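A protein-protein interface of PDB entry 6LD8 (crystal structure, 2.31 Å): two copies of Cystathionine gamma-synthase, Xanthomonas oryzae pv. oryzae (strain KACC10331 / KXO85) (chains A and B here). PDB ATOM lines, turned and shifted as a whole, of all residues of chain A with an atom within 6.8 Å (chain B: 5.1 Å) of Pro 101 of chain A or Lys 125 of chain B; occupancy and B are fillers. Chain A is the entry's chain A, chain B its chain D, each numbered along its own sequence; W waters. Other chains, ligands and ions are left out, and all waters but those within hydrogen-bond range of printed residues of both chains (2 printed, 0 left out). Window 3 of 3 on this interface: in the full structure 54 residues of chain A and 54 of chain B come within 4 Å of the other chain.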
ATOM      1  N   VAL A  94      11.639  22.750  -4.677  1.00  0.00           N
ATOM      2  CA  VAL A  94      10.455  23.003  -3.808  1.00  0.00           C
ATOM      3  C   VAL A  94      10.695  22.359  -2.420  1.00  0.00           C
ATOM      4  O   VAL A  94      10.472  23.027  -1.412  1.00  0.00           O
ATOM      5  CB  VAL A  94       9.144  22.522  -4.472  1.00  0.00           C
ATOM      6  CG1 VAL A  94       7.954  22.546  -3.493  1.00  0.00           C
ATOM      7  CG2 VAL A  94       8.828  23.350  -5.702  1.00  0.00           C
ATOM      8  N   LEU A  95      11.131  21.120  -2.364  1.00  0.00           N
ATOM      9  CA  LEU A  95      11.395  20.436  -1.073  1.00  0.00           C
ATOM     10  C   LEU A  95      12.401  21.248  -0.242  1.00  0.00           C
ATOM     11  O   LEU A  95      12.116  21.467   0.924  1.00  0.00           O
ATOM     12  CB  LEU A  95      11.915  19.033  -1.329  1.00  0.00           C
ATOM     13  CG  LEU A  95      10.977  18.159  -2.135  1.00  0.00           C
ATOM     14  CD1 LEU A  95      11.471  16.734  -2.159  1.00  0.00           C
ATOM     15  CD2 LEU A  95       9.575  18.227  -1.590  1.00  0.00           C
ATOM     16  N   ASN A  96      13.467  21.775  -0.836  1.00  0.00           N
ATOM     17  CA  ASN A  96      14.481  22.589  -0.118  1.00  0.00           C
ATOM     18  C   ASN A  96      13.908  23.965   0.255  1.00  0.00           C
ATOM     19  O   ASN A  96      14.288  24.516   1.310  1.00  0.00           O
ATOM     20  CB  ASN A  96      15.782  22.710  -0.924  1.00  0.00           C
ATOM     21  CG  ASN A  96      16.704  21.523  -0.751  1.00  0.00           C
ATOM     22  OD1 ASN A  96      17.550  21.519   0.152  1.00  0.00           O
ATOM     23  ND2 ASN A  96      16.532  20.499  -1.579  1.00  0.00           N
ATOM     24  N   ALA A  97      13.071  24.588  -0.557  1.00  0.00           N
ATOM     25  CA  ALA A  97      12.647  25.961  -0.234  1.00  0.00           C
ATOM     26  C   ALA A  97      11.591  25.957   0.877  1.00  0.00           C
ATOM     27  O   ALA A  97      11.424  26.995   1.509  1.00  0.00           O
ATOM     28  CB  ALA A  97      12.096  26.613  -1.464  1.00  0.00           C
ATOM     29  N   VAL A  98      10.814  24.881   1.014  1.00  0.00           N
ATOM     30  CA  VAL A  98       9.546  24.883   1.797  1.00  0.00           C
ATOM     31  C   VAL A  98       9.678  24.029   3.068  1.00  0.00           C
ATOM     32  O   VAL A  98       9.085  24.398   4.050  1.00  0.00           O
ATOM     33  CB  VAL A  98       8.394  24.389   0.905  1.00  0.00           C
ATOM     34  CG1 VAL A  98       7.162  23.981   1.696  1.00  0.00           C
ATOM     35  CG2 VAL A  98       8.037  25.446  -0.101  1.00  0.00           C
ATOM     36  N   LEU A  99      10.300  22.862   3.004  1.00  0.00           N
ATOM     37  CA  LEU A  99      10.372  21.894   4.118  1.00  0.00           C
ATOM     38  C   LEU A  99      11.680  22.089   4.898  1.00  0.00           C
ATOM     39  O   LEU A  99      12.603  22.656   4.327  1.00  0.00           O
ATOM     40  CB  LEU A  99      10.304  20.471   3.556  1.00  0.00           C
ATOM     41  CG  LEU A  99       9.016  20.148   2.818  1.00  0.00           C
ATOM     42  CD1 LEU A  99       9.052  18.778   2.162  1.00  0.00           C
ATOM     43  CD2 LEU A  99       7.842  20.267   3.768  1.00  0.00           C
ATOM     44  N   GLN A 100      11.691  21.683   6.176  1.00  0.00           N
ATOM     45  CA  GLN A 100      12.880  21.449   7.046  1.00  0.00           C
ATOM     46  C   GLN A 100      12.582  20.263   7.960  1.00  0.00           C
ATOM     47  O   GLN A 100      11.432  19.849   8.081  1.00  0.00           O
ATOM     48  CB  GLN A 100      13.226  22.687   7.875  1.00  0.00           C
ATOM     49  CG  GLN A 100      12.128  23.150   8.819  1.00  0.00           C
ATOM     50  CD  GLN A 100      12.548  24.342   9.649  1.00  0.00           C
ATOM     51  OE1 GLN A 100      11.719  25.062  10.174  1.00  0.00           O
ATOM     52  NE2 GLN A 100      13.845  24.570   9.788  1.00  0.00           N
ATOM     53  N   PRO A 101      13.586  19.669   8.637  1.00  0.00           N
ATOM     54  CA  PRO A 101      13.333  18.549   9.548  1.00  0.00           C
ATOM     55  C   PRO A 101      12.270  18.897  10.593  1.00  0.00           C
ATOM     56  O   PRO A 101      12.126  20.074  11.037  1.00  0.00           O
ATOM     57  CB  PRO A 101      14.711  18.247  10.146  1.00  0.00           C
ATOM     58  CG  PRO A 101      15.670  18.718   9.055  1.00  0.00           C
ATOM     59  CD  PRO A 101      15.013  19.982   8.527  1.00  0.00           C
ATOM     60  N   GLY A 102      11.430  17.903  10.850  1.00  0.00           N
ATOM     61  CA  GLY A 102      10.229  18.090  11.681  1.00  0.00           C
ATOM     62  C   GLY A 102       8.980  18.403  10.870  1.00  0.00           C
ATOM     63  O   GLY A 102       7.905  18.159  11.424  1.00  0.00           O
ATOM     64  N   ASP A 103       9.084  18.906   9.619  1.00  0.00           N
ATOM     65  CA  ASP A 103       7.909  19.113   8.715  1.00  0.00           C
ATOM     66  C   ASP A 103       7.434  17.775   8.136  1.00  0.00           C
ATOM     67  O   ASP A 103       8.248  16.806   8.015  1.00  0.00           O
ATOM     68  CB  ASP A 103       8.178  20.105   7.598  1.00  0.00           C
ATOM     69  CG  ASP A 103       8.302  21.539   8.067  1.00  0.00           C
ATOM     70  OD1 ASP A 103       7.760  21.836   9.135  1.00  0.00           O
ATOM     71  OD2 ASP A 103       8.928  22.345   7.334  1.00  0.00           O
ATOM     72  N   GLY A 126      15.859  11.903   7.064  1.00  0.00           N
ATOM     73  CA  GLY A 126      15.249  12.775   8.085  1.00  0.00           C
ATOM     74  C   GLY A 126      15.123  14.217   7.646  1.00  0.00           C
ATOM     75  O   GLY A 126      14.983  15.066   8.545  1.00  0.00           O
ATOM     76  N   HIS A 127      15.056  14.519   6.335  1.00  0.00           N
ATOM     77  CA  HIS A 127      14.871  15.929   5.891  1.00  0.00           C
ATOM     78  C   HIS A 127      13.432  16.370   6.192  1.00  0.00           C
ATOM     79  O   HIS A 127      13.186  17.592   6.330  1.00  0.00           O
ATOM     80  CB  HIS A 127      15.257  16.101   4.422  1.00  0.00           C
ATOM     81  CG  HIS A 127      16.724  16.083   4.209  1.00  0.00           C
ATOM     82  ND1 HIS A 127      17.294  16.534   3.042  1.00  0.00           N
ATOM     83  CD2 HIS A 127      17.739  15.708   5.027  1.00  0.00           C
ATOM     84  CE1 HIS A 127      18.602  16.422   3.146  1.00  0.00           C
ATOM     85  NE2 HIS A 127      18.898  15.925   4.346  1.00  0.00           N
ATOM     86  N   PHE A 128      12.508  15.413   6.251  1.00  0.00           N
ATOM     87  CA  PHE A 128      11.069  15.662   6.546  1.00  0.00           C
ATOM     88  C   PHE A 128      10.430  14.295   6.824  1.00  0.00           C
ATOM     89  O   PHE A 128      11.100  13.257   6.575  1.00  0.00           O
ATOM     90  CB  PHE A 128      10.411  16.477   5.410  1.00  0.00           C
ATOM     91  CG  PHE A 128      10.681  15.918   4.033  1.00  0.00           C
ATOM     92  CD1 PHE A 128      10.096  14.734   3.618  1.00  0.00           C
ATOM     93  CD2 PHE A 128      11.617  16.505   3.202  1.00  0.00           C
ATOM     94  CE1 PHE A 128      10.407  14.179   2.383  1.00  0.00           C
ATOM     95  CE2 PHE A 128      11.928  15.939   1.983  1.00  0.00           C
ATOM     96  CZ  PHE A 128      11.351  14.773   1.579  1.00  0.00           C
ATOM     97  N   ALA A 129       9.212  14.297   7.372  1.00  0.00           N
ATOM     98  CA  ALA A 129       8.407  13.061   7.481  1.00  0.00           C
ATOM     99  C   ALA A 129       7.500  12.982   6.257  1.00  0.00           C
ATOM    100  O   ALA A 129       7.003  14.046   5.761  1.00  0.00           O
ATOM    101  CB  ALA A 129       7.611  13.032   8.766  1.00  0.00           C
ATOM    102  N   TRP A 236      16.856  29.983  -3.410  1.00  0.00           N
ATOM    103  CA  TRP A 236      17.290  28.593  -3.182  1.00  0.00           C
ATOM    104  C   TRP A 236      17.856  28.003  -4.475  1.00  0.00           C
ATOM    105  O   TRP A 236      18.782  27.165  -4.392  1.00  0.00           O
ATOM    106  CB  TRP A 236      16.146  27.764  -2.633  1.00  0.00           C
ATOM    107  CG  TRP A 236      15.991  27.959  -1.172  1.00  0.00           C
ATOM    108  CD1 TRP A 236      15.112  28.786  -0.546  1.00  0.00           C
ATOM    109  CD2 TRP A 236      16.789  27.360  -0.152  1.00  0.00           C
ATOM    110  NE1 TRP A 236      15.300  28.738   0.799  1.00  0.00           N
ATOM    111  CE2 TRP A 236      16.314  27.864   1.078  1.00  0.00           C
ATOM    112  CE3 TRP A 236      17.873  26.474  -0.154  1.00  0.00           C
ATOM    113  CZ2 TRP A 236      16.904  27.530   2.300  1.00  0.00           C
ATOM    114  CZ3 TRP A 236      18.436  26.111   1.055  1.00  0.00           C
ATOM    115  CH2 TRP A 236      17.951  26.629   2.264  1.00  0.00           C
ATOM    116  N   ALA B 121      23.115  27.966   5.099  1.00  0.00           N
ATOM    117  CA  ALA B 121      21.650  27.835   4.893  1.00  0.00           C
ATOM    118  C   ALA B 121      21.228  26.411   5.263  1.00  0.00           C
ATOM    119  O   ALA B 121      20.211  26.271   5.976  1.00  0.00           O
ATOM    120  CB  ALA B 121      21.245  28.231   3.489  1.00  0.00           C
ATOM    121  N   LEU B 122      21.999  25.399   4.890  1.00  0.00           N
ATOM    122  CA  LEU B 122      21.635  23.978   5.166  1.00  0.00           C
ATOM    123  C   LEU B 122      21.903  23.544   6.622  1.00  0.00           C
ATOM    124  O   LEU B 122      21.229  22.569   7.116  1.00  0.00           O
ATOM    125  CB  LEU B 122      22.415  23.083   4.208  1.00  0.00           C
ATOM    126  CG  LEU B 122      22.069  23.199   2.718  1.00  0.00           C
ATOM    127  CD1 LEU B 122      22.833  22.131   1.942  1.00  0.00           C
ATOM    128  CD2 LEU B 122      20.555  23.055   2.458  1.00  0.00           C
ATOM    129  N   ALA B 123      22.892  24.158   7.272  1.00  0.00           N
ATOM    130  CA  ALA B 123      23.183  23.937   8.711  1.00  0.00           C
ATOM    131  C   ALA B 123      22.043  24.533   9.544  1.00  0.00           C
ATOM    132  O   ALA B 123      21.672  23.917  10.547  1.00  0.00           O
ATOM    133  CB  ALA B 123      24.516  24.561   9.091  1.00  0.00           C
ATOM    134  N   LYS B 124      21.539  25.698   9.145  1.00  0.00           N
ATOM    135  CA  LYS B 124      20.418  26.394   9.824  1.00  0.00           C
ATOM    136  C   LYS B 124      19.170  25.511   9.791  1.00  0.00           C
ATOM    137  O   LYS B 124      18.456  25.517  10.762  1.00  0.00           O
ATOM    138  CB  LYS B 124      20.086  27.719   9.152  1.00  0.00           C
ATOM    139  CG  LYS B 124      20.539  28.974   9.885  1.00  0.00           C
ATOM    140  CD  LYS B 124      19.588  30.147   9.654  1.00  0.00           C
ATOM    141  CE  LYS B 124      18.124  29.726   9.697  1.00  0.00           C
ATOM    142  NZ  LYS B 124      17.208  30.854   9.426  1.00  0.00           N
ATOM    143  N   LYS B 125      18.943  24.760   8.716  1.00  0.00           N
ATOM    144  CA  LYS B 125      17.791  23.834   8.596  1.00  0.00           C
ATOM    145  C   LYS B 125      18.045  22.567   9.394  1.00  0.00           C
ATOM    146  O   LYS B 125      17.118  21.833   9.602  1.00  0.00           O
ATOM    147  CB  LYS B 125      17.594  23.331   7.166  1.00  0.00           C
ATOM    148  CG  LYS B 125      17.023  24.346   6.206  1.00  0.00           C
ATOM    149  CD  LYS B 125      16.852  23.720   4.871  1.00  0.00           C
ATOM    150  CE  LYS B 125      15.505  23.980   4.255  1.00  0.00           C
ATOM    151  NZ  LYS B 125      15.372  23.037   3.127  1.00  0.00           N
ATOM    152  N   GLY B 126      19.289  22.221   9.654  1.00  0.00           N
ATOM    153  CA  GLY B 126      19.589  21.008  10.429  1.00  0.00           C
ATOM    154  C   GLY B 126      19.955  19.824   9.579  1.00  0.00           C
ATOM    155  O   GLY B 126      19.867  18.693  10.127  1.00  0.00           O
ATOM    156  N   HIS B 127      20.467  20.031   8.349  1.00  0.00           N
ATOM    157  CA  HIS B 127      20.885  18.883   7.502  1.00  0.00           C
ATOM    158  C   HIS B 127      22.173  18.298   8.078  1.00  0.00           C
ATOM    159  O   HIS B 127      22.460  17.095   7.840  1.00  0.00           O
ATOM    160  CB  HIS B 127      21.008  19.267   6.026  1.00  0.00           C
ATOM    161  CG  HIS B 127      19.685  19.495   5.396  1.00  0.00           C
ATOM    162  ND1 HIS B 127      19.517  19.537   4.026  1.00  0.00           N
ATOM    163  CD2 HIS B 127      18.459  19.653   5.951  1.00  0.00           C
ATOM    164  CE1 HIS B 127      18.243  19.752   3.772  1.00  0.00           C
ATOM    165  NE2 HIS B 127      17.580  19.827   4.929  1.00  0.00           N
HETATM  166  O   HOH W   1      21.566  15.877   5.464  1.00  0.00           O
HETATM  167  O   HOH W   2      14.677  19.565   5.009  1.00  0.00           O
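Pro 101 of chain A touches one residue of chain B.
Of chain A, only Asn 96, Leu 99 and Pro 101 come within 4 Å of Lys 125 of chain B.
Of the printed residues of chain A, His 127 of chain B touches His 127.
Of the printed residues of chain B, Trp 236 of chain A touches Ala 121 (3.9 Å) and Leu 122 (3.97 Å).
Printed residues of chain B within 4 Å of Asn 96 of chain A: Lys 125.
Ala 129 of chain A touches none of the printed residues of chain B.
Gly 102 of chain A touches none of the printed residues of chain B.
Water W2 lies within hydrogen-bond range of O of His 127 of chain A and NE2 of His 127 of chain B.
Water W1 bridges the backbone carbonyl oxygen of His 127 of chain B and a ring nitrogen (NE2) of His 127 of chain A.
His 127 of chain B touches its own counterpart, His 127 of chain A.
Among the printed residues, merely in contact across the chains: Pro 101 of chain A with Lys 125 of chain B (3.0 Å), His 127 of chain A with His 127 of chain B (3.4 Å), Trp 236 of chain A with Ala 121 of chain B (3.9 Å) and Trp 236 of chain A with Leu 122 of chain B (3.97 Å).
O of Asn 96 of chain A sits at hydrogen-bond distance from NZ of Lys 125 of chain B.
NZ of Lys 125 of chain B sits at hydrogen-bond distance from O of Leu 99 of chain A.
Of the 7 printed residues of chain B, 4 touch a printed residue of chain A.
Hydrophobic or aromatic side chains of chain B within 4 Å of the printed part of chain A: Ala 121, Leu 122 and His 127.
Of the 15 printed residues of chain A, 5 touch a printed residue of chain B.
Hydrophobic or aromatic side chains of chain A that line the printed part of chain B: Pro 101, His 127 and Trp 236.
The backbone carbonyl oxygen (O) of Leu 122 of chain B sits at hydrogen-bond distance from the backbone NH (N) of His 127 of chain B (2.9 Å).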
